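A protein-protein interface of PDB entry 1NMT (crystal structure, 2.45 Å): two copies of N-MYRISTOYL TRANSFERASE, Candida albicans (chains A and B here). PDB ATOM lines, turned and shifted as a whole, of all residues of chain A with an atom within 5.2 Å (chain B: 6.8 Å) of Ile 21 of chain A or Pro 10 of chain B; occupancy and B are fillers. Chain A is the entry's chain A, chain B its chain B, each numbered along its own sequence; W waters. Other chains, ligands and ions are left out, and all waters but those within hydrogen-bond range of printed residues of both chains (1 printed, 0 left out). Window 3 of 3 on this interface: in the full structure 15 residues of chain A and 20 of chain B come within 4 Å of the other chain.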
ATOM      1  N   PRO A  19     -19.092  25.617  24.567  1.00  0.00           N
ATOM      2  CA  PRO A  19     -19.414  24.211  24.838  1.00  0.00           C
ATOM      3  C   PRO A  19     -18.459  23.664  25.887  1.00  0.00           C
ATOM      4  O   PRO A  19     -17.341  24.162  26.030  1.00  0.00           O
ATOM      5  CB  PRO A  19     -19.215  23.517  23.481  1.00  0.00           C
ATOM      6  CG  PRO A  19     -19.095  24.633  22.455  1.00  0.00           C
ATOM      7  CD  PRO A  19     -18.557  25.823  23.208  1.00  0.00           C
ATOM      8  N   LEU A  20     -18.897  22.653  26.625  1.00  0.00           N
ATOM      9  CA  LEU A  20     -18.030  22.049  27.620  1.00  0.00           C
ATOM     10  C   LEU A  20     -18.022  20.546  27.415  1.00  0.00           C
ATOM     11  O   LEU A  20     -18.952  19.988  26.828  1.00  0.00           O
ATOM     12  CB  LEU A  20     -18.552  22.332  29.026  1.00  0.00           C
ATOM     13  CG  LEU A  20     -18.372  23.733  29.592  1.00  0.00           C
ATOM     14  CD1 LEU A  20     -19.185  23.898  30.895  1.00  0.00           C
ATOM     15  CD2 LEU A  20     -16.894  23.951  29.825  1.00  0.00           C
ATOM     16  N   ILE A  21     -16.963  19.900  27.881  1.00  0.00           N
ATOM     17  CA  ILE A  21     -16.879  18.450  27.856  1.00  0.00           C
ATOM     18  C   ILE A  21     -18.249  18.095  28.489  1.00  0.00           C
ATOM     19  O   ILE A  21     -18.659  18.727  29.480  1.00  0.00           O
ATOM     20  CB  ILE A  21     -15.696  18.015  28.762  1.00  0.00           C
ATOM     21  CG1 ILE A  21     -14.393  18.054  27.947  1.00  0.00           C
ATOM     22  CG2 ILE A  21     -15.945  16.662  29.381  1.00  0.00           C
ATOM     23  CD1 ILE A  21     -13.085  18.181  28.801  1.00  0.00           C
ATOM     24  N   SER A  22     -18.967  17.129  27.911  1.00  0.00           N
ATOM     25  CA  SER A  22     -20.317  16.783  28.395  1.00  0.00           C
ATOM     26  C   SER A  22     -20.480  16.521  29.902  1.00  0.00           C
ATOM     27  O   SER A  22     -21.580  16.651  30.429  1.00  0.00           O
ATOM     28  CB  SER A  22     -20.891  15.600  27.594  1.00  0.00           C
ATOM     29  OG  SER A  22     -20.472  14.352  28.138  1.00  0.00           O
ATOM     30  N   ASP A  23     -19.402  16.175  30.597  1.00  0.00           N
ATOM     31  CA  ASP A  23     -19.464  15.910  32.038  1.00  0.00           C
ATOM     32  C   ASP A  23     -19.755  17.166  32.862  1.00  0.00           C
ATOM     33  O   ASP A  23     -20.205  17.085  34.017  1.00  0.00           O
ATOM     34  CB  ASP A  23     -18.125  15.354  32.535  1.00  0.00           C
ATOM     35  CG  ASP A  23     -17.932  13.908  32.182  1.00  0.00           C
ATOM     36  OD1 ASP A  23     -18.948  13.265  31.848  1.00  0.00           O
ATOM     37  OD2 ASP A  23     -16.773  13.424  32.241  1.00  0.00           O
ATOM     38  N   PHE A  24     -19.501  18.332  32.279  1.00  0.00           N
ATOM     39  CA  PHE A  24     -19.656  19.567  33.026  1.00  0.00           C
ATOM     40  C   PHE A  24     -20.636  20.549  32.447  1.00  0.00           C
ATOM     41  O   PHE A  24     -21.103  20.410  31.316  1.00  0.00           O
ATOM     42  CB  PHE A  24     -18.285  20.264  33.172  1.00  0.00           C
ATOM     43  CG  PHE A  24     -17.165  19.329  33.550  1.00  0.00           C
ATOM     44  CD1 PHE A  24     -17.091  18.803  34.839  1.00  0.00           C
ATOM     45  CD2 PHE A  24     -16.177  18.979  32.621  1.00  0.00           C
ATOM     46  CE1 PHE A  24     -16.038  17.936  35.202  1.00  0.00           C
ATOM     47  CE2 PHE A  24     -15.127  18.114  32.973  1.00  0.00           C
ATOM     48  CZ  PHE A  24     -15.059  17.595  34.259  1.00  0.00           C
ATOM     49  N   LYS A 127      -7.643  18.477  32.207  1.00  0.00           N
ATOM     50  CA  LYS A 127      -8.774  18.623  31.292  1.00  0.00           C
ATOM     51  C   LYS A 127      -8.544  19.893  30.456  1.00  0.00           C
ATOM     52  O   LYS A 127      -9.283  20.163  29.499  1.00  0.00           O
ATOM     53  CB  LYS A 127     -10.114  18.706  32.062  1.00  0.00           C
ATOM     54  CG  LYS A 127     -10.552  17.410  32.749  1.00  0.00           C
ATOM     55  CD  LYS A 127     -10.900  16.365  31.719  1.00  0.00           C
ATOM     56  CE  LYS A 127     -11.326  15.018  32.322  1.00  0.00           C
ATOM     57  NZ  LYS A 127     -12.311  14.353  31.372  1.00  0.00           N
ATOM     58  N   LYS B   8     -19.522  22.634  16.776  1.00  0.00           N
ATOM     59  CA  LYS B   8     -20.542  21.969  17.567  1.00  0.00           C
ATOM     60  C   LYS B   8     -20.010  21.752  18.969  1.00  0.00           C
ATOM     61  O   LYS B   8     -18.933  22.230  19.323  1.00  0.00           O
ATOM     62  CB  LYS B   8     -20.940  20.619  16.942  1.00  0.00           C
ATOM     63  CG  LYS B   8     -19.806  19.827  16.291  1.00  0.00           C
ATOM     64  CD  LYS B   8     -20.329  18.562  15.601  1.00  0.00           C
ATOM     65  CE  LYS B   8     -19.231  17.540  15.376  1.00  0.00           C
ATOM     66  NZ  LYS B   8     -19.648  16.442  14.462  1.00  0.00           N
ATOM     67  N   THR B   9     -20.773  21.018  19.763  1.00  0.00           N
ATOM     68  CA  THR B   9     -20.382  20.728  21.127  1.00  0.00           C
ATOM     69  C   THR B   9     -20.085  19.246  21.285  1.00  0.00           C
ATOM     70  O   THR B   9     -20.467  18.440  20.437  1.00  0.00           O
ATOM     71  CB  THR B   9     -21.504  21.109  22.072  1.00  0.00           C
ATOM     72  OG1 THR B   9     -22.459  20.044  22.132  1.00  0.00           O
ATOM     73  CG2 THR B   9     -22.194  22.366  21.566  1.00  0.00           C
ATOM     74  N   PRO B  10     -19.365  18.868  22.350  1.00  0.00           N
ATOM     75  CA  PRO B  10     -19.057  17.449  22.554  1.00  0.00           C
ATOM     76  C   PRO B  10     -20.314  16.594  22.449  1.00  0.00           C
ATOM     77  O   PRO B  10     -20.274  15.447  21.989  1.00  0.00           O
ATOM     78  CB  PRO B  10     -18.434  17.421  23.942  1.00  0.00           C
ATOM     79  CG  PRO B  10     -17.775  18.786  24.049  1.00  0.00           C
ATOM     80  CD  PRO B  10     -18.747  19.719  23.382  1.00  0.00           C
ATOM     81  N   GLU B  11     -21.429  17.184  22.864  1.00  0.00           N
ATOM     82  CA  GLU B  11     -22.746  16.556  22.822  1.00  0.00           C
ATOM     83  C   GLU B  11     -23.124  16.086  21.423  1.00  0.00           C
ATOM     84  O   GLU B  11     -23.656  14.995  21.264  1.00  0.00           O
ATOM     85  CB  GLU B  11     -23.804  17.558  23.279  1.00  0.00           C
ATOM     86  CG  GLU B  11     -23.942  17.663  24.762  1.00  0.00           C
ATOM     87  CD  GLU B  11     -24.134  16.317  25.385  1.00  0.00           C
ATOM     88  OE1 GLU B  11     -23.113  15.607  25.549  1.00  0.00           O
ATOM     89  OE2 GLU B  11     -25.298  15.976  25.701  1.00  0.00           O
ATOM     90  N   ASP B  12     -22.876  16.922  20.419  1.00  0.00           N
ATOM     91  CA  ASP B  12     -23.213  16.596  19.039  1.00  0.00           C
ATOM     92  C   ASP B  12     -22.290  15.530  18.440  1.00  0.00           C
ATOM     93  O   ASP B  12     -22.413  15.167  17.267  1.00  0.00           O
ATOM     94  CB  ASP B  12     -23.152  17.864  18.175  1.00  0.00           C
ATOM     95  CG  ASP B  12     -24.054  18.986  18.700  1.00  0.00           C
ATOM     96  OD1 ASP B  12     -25.070  18.659  19.369  1.00  0.00           O
ATOM     97  OD2 ASP B  12     -23.737  20.183  18.440  1.00  0.00           O
ATOM     98  N   VAL B  13     -21.359  15.032  19.244  1.00  0.00           N
ATOM     99  CA  VAL B  13     -20.425  14.033  18.762  1.00  0.00           C
ATOM    100  C   VAL B  13     -20.887  12.623  19.127  1.00  0.00           C
ATOM    101  O   VAL B  13     -21.235  12.343  20.271  1.00  0.00           O
ATOM    102  CB  VAL B  13     -18.987  14.281  19.355  1.00  0.00           C
ATOM    103  CG1 VAL B  13     -18.049  13.125  19.001  1.00  0.00           C
ATOM    104  CG2 VAL B  13     -18.416  15.585  18.822  1.00  0.00           C
ATOM    105  N   PRO B  14     -20.878  11.714  18.151  1.00  0.00           N
ATOM    106  CA  PRO B  14     -21.297  10.320  18.384  1.00  0.00           C
ATOM    107  C   PRO B  14     -20.629   9.711  19.628  1.00  0.00           C
ATOM    108  O   PRO B  14     -19.410   9.785  19.801  1.00  0.00           O
ATOM    109  CB  PRO B  14     -20.893   9.598  17.090  1.00  0.00           C
ATOM    110  CG  PRO B  14     -20.881  10.683  16.034  1.00  0.00           C
ATOM    111  CD  PRO B  14     -20.473  11.966  16.751  1.00  0.00           C
ATOM    112  N   ASN B  15     -21.420   9.086  20.487  1.00  0.00           N
ATOM    113  CA  ASN B  15     -20.875   8.521  21.716  1.00  0.00           C
ATOM    114  C   ASN B  15     -20.133   7.226  21.529  1.00  0.00           C
ATOM    115  O   ASN B  15     -19.345   6.836  22.388  1.00  0.00           O
ATOM    116  CB  ASN B  15     -21.985   8.333  22.767  1.00  0.00           C
ATOM    117  CG  ASN B  15     -22.759   9.618  23.026  1.00  0.00           C
ATOM    118  OD1 ASN B  15     -22.166  10.671  23.268  1.00  0.00           O
ATOM    119  ND2 ASN B  15     -24.088   9.541  22.966  1.00  0.00           N
ATOM    120  N   ASN B 142     -12.717  15.180  19.925  1.00  0.00           N
ATOM    121  CA  ASN B 142     -13.841  16.133  19.829  1.00  0.00           C
ATOM    122  C   ASN B 142     -14.704  15.973  21.082  1.00  0.00           C
ATOM    123  O   ASN B 142     -15.273  16.939  21.582  1.00  0.00           O
ATOM    124  CB  ASN B 142     -14.723  15.863  18.591  1.00  0.00           C
ATOM    125  CG  ASN B 142     -14.057  16.281  17.297  1.00  0.00           C
ATOM    126  OD1 ASN B 142     -14.598  16.088  16.212  1.00  0.00           O
ATOM    127  ND2 ASN B 142     -12.859  16.851  17.407  1.00  0.00           N
ATOM    128  N   LYS B 143     -14.781  14.747  21.588  1.00  0.00           N
ATOM    129  CA  LYS B 143     -15.563  14.451  22.786  1.00  0.00           C
ATOM    130  C   LYS B 143     -14.934  15.172  23.977  1.00  0.00           C
ATOM    131  O   LYS B 143     -15.607  15.508  24.960  1.00  0.00           O
ATOM    132  CB  LYS B 143     -15.594  12.932  23.043  1.00  0.00           C
ATOM    133  CG  LYS B 143     -16.946  12.384  23.513  1.00  0.00           C
ATOM    134  CD  LYS B 143     -18.056  12.588  22.484  1.00  0.00           C
ATOM    135  CE  LYS B 143     -19.340  11.908  22.961  1.00  0.00           C
ATOM    136  NZ  LYS B 143     -20.561  12.763  22.879  1.00  0.00           N
ATOM    137  N   GLN B 144     -13.631  15.401  23.891  1.00  0.00           N
ATOM    138  CA  GLN B 144     -12.931  16.117  24.949  1.00  0.00           C
ATOM    139  C   GLN B 144     -12.893  17.607  24.627  1.00  0.00           C
ATOM    140  O   GLN B 144     -12.083  18.348  25.181  1.00  0.00           O
ATOM    141  CB  GLN B 144     -11.500  15.606  25.100  1.00  0.00           C
ATOM    142  CG  GLN B 144     -11.415  14.227  25.678  1.00  0.00           C
ATOM    143  CD  GLN B 144     -12.225  14.086  26.934  1.00  0.00           C
ATOM    144  OE1 GLN B 144     -13.104  13.242  26.990  1.00  0.00           O
ATOM    145  NE2 GLN B 144     -11.939  14.915  27.952  1.00  0.00           N
ATOM    146  N   ASN B 145     -13.760  18.033  23.715  1.00  0.00           N
ATOM    147  CA  ASN B 145     -13.836  19.437  23.339  1.00  0.00           C
ATOM    148  C   ASN B 145     -12.558  19.993  22.680  1.00  0.00           C
ATOM    149  O   ASN B 145     -12.208  21.145  22.905  1.00  0.00           O
ATOM    150  CB  ASN B 145     -14.196  20.284  24.571  1.00  0.00           C
ATOM    151  CG  ASN B 145     -14.921  21.577  24.206  1.00  0.00           C
ATOM    152  OD1 ASN B 145     -15.481  21.726  23.102  1.00  0.00           O
ATOM    153  ND2 ASN B 145     -14.911  22.525  25.141  1.00  0.00           N
ATOM    154  N   ILE B 146     -11.842  19.176  21.901  1.00  0.00           N
ATOM    155  CA  ILE B 146     -10.658  19.661  21.191  1.00  0.00           C
ATOM    156  C   ILE B 146     -11.105  19.553  19.749  1.00  0.00           C
ATOM    157  O   ILE B 146     -11.605  18.501  19.347  1.00  0.00           O
ATOM    158  CB  ILE B 146      -9.407  18.791  21.458  1.00  0.00           C
ATOM    159  CG1 ILE B 146      -9.066  18.829  22.945  1.00  0.00           C
ATOM    160  CG2 ILE B 146      -8.187  19.347  20.708  1.00  0.00           C
ATOM    161  CD1 ILE B 146      -8.604  20.194  23.436  1.00  0.00           C
ATOM    162  N   TRP B 147     -10.944  20.630  18.976  1.00  0.00           N
ATOM    163  CA  TRP B 147     -11.442  20.664  17.605  1.00  0.00           C
ATOM    164  C   TRP B 147     -10.440  20.861  16.467  1.00  0.00           C
ATOM    165  O   TRP B 147     -10.833  20.949  15.306  1.00  0.00           O
ATOM    166  CB  TRP B 147     -12.582  21.718  17.513  1.00  0.00           C
ATOM    167  CG  TRP B 147     -13.659  21.466  18.535  1.00  0.00           C
ATOM    168  CD1 TRP B 147     -13.676  21.911  19.840  1.00  0.00           C
ATOM    169  CD2 TRP B 147     -14.797  20.588  18.395  1.00  0.00           C
ATOM    170  NE1 TRP B 147     -14.748  21.357  20.514  1.00  0.00           N
ATOM    171  CE2 TRP B 147     -15.450  20.544  19.656  1.00  0.00           C
ATOM    172  CE3 TRP B 147     -15.322  19.837  17.333  1.00  0.00           C
ATOM    173  CZ2 TRP B 147     -16.599  19.780  19.881  1.00  0.00           C
ATOM    174  CZ3 TRP B 147     -16.468  19.077  17.557  1.00  0.00           C
ATOM    175  CH2 TRP B 147     -17.093  19.057  18.827  1.00  0.00           C
HETATM  176  O   HOH W   1     -17.835  14.748  26.446  1.00  0.00           O
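OG1 of Thr 9 of chain B sits close to N of Glu 11 of chain B (3.1 Å).
O of Pro 10 of chain B lies within hydrogen-bond range of NZ of Lys 143 of chain B, at 2.8 Å.
The side-chain carboxylate (OD2) of Asp 12 of chain B is in hydrogen-bond range of the backbone NH (N) of Thr 9 of chain B (3.4 Å).
The indole nitrogen (NE1) of Trp 147 of chain B sits at hydrogen-bond distance from the side-chain amide oxygen (OD1) of Asn 145 of chain B, at 2.7 Å.
Water W1 bridges O of Lys 143 of chain B (2.8 Å) and N of Ser 22 of chain A (3.0 Å).
Printed residues of chain B that touch a printed residue of chain A: Lys 8, Thr 9, Pro 10, Glu 11, Gln 144 and Asn 145.
Hydrophobic or aromatic side chains of chain B within 4 Å of the printed part of chain A: Pro 10.
Of the printed residues of chain B, Pro 19 of chain A touches Lys 8 (3.95 Å), Thr 9 (3.6 Å), Pro 10 (3.8 Å) and Asn 145 (3.1 Å).
Printed residues of chain B within 4 Å of Ile 21 of chain A: Pro 10 and Gln 144.
Printed residues of chain B within 4 Å of Ser 22 of chain A: Glu 11.
Printed residues of chain A within 4 Å of Pro 10 of chain B: Pro 19, Leu 20 and Ile 21.
The nearest printed residue of chain A that does not touch Lys 8 of chain B is Leu 20 of chain A (7.3 Å).
No position is printed for both chains.
Pro 19 of chain A touches Lys 8 of chain B (CG to O, 3.95 Å).
CB of Pro 19 of chain A touches CB of Thr 9 of chain B, at 3.6 Å.
Pro 10 of chain B touches Pro 19 of chain A.
O of Leu 20 of chain A touches CG of Pro 10 of chain B (3.2 Å).
Pro 10 of chain B touches Ile 21 of chain A (CG to CA, 3.9 Å).
Ile 21 of chain A touches Gln 144 of chain B (CD1 to NE2, 3.6 Å).
Glu 11 of chain B touches Ser 22 of chain A.
The side-chain amino group of Lys 127 of chain A lies close to the side-chain amide nitrogen of Gln 144 of chain B (3.5 Å).
The side-chain amide nitrogen (ND2) of Asn 145 of chain B sits at hydrogen-bond distance from the backbone carbonyl oxygen (O) of Pro 19 of chain A.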
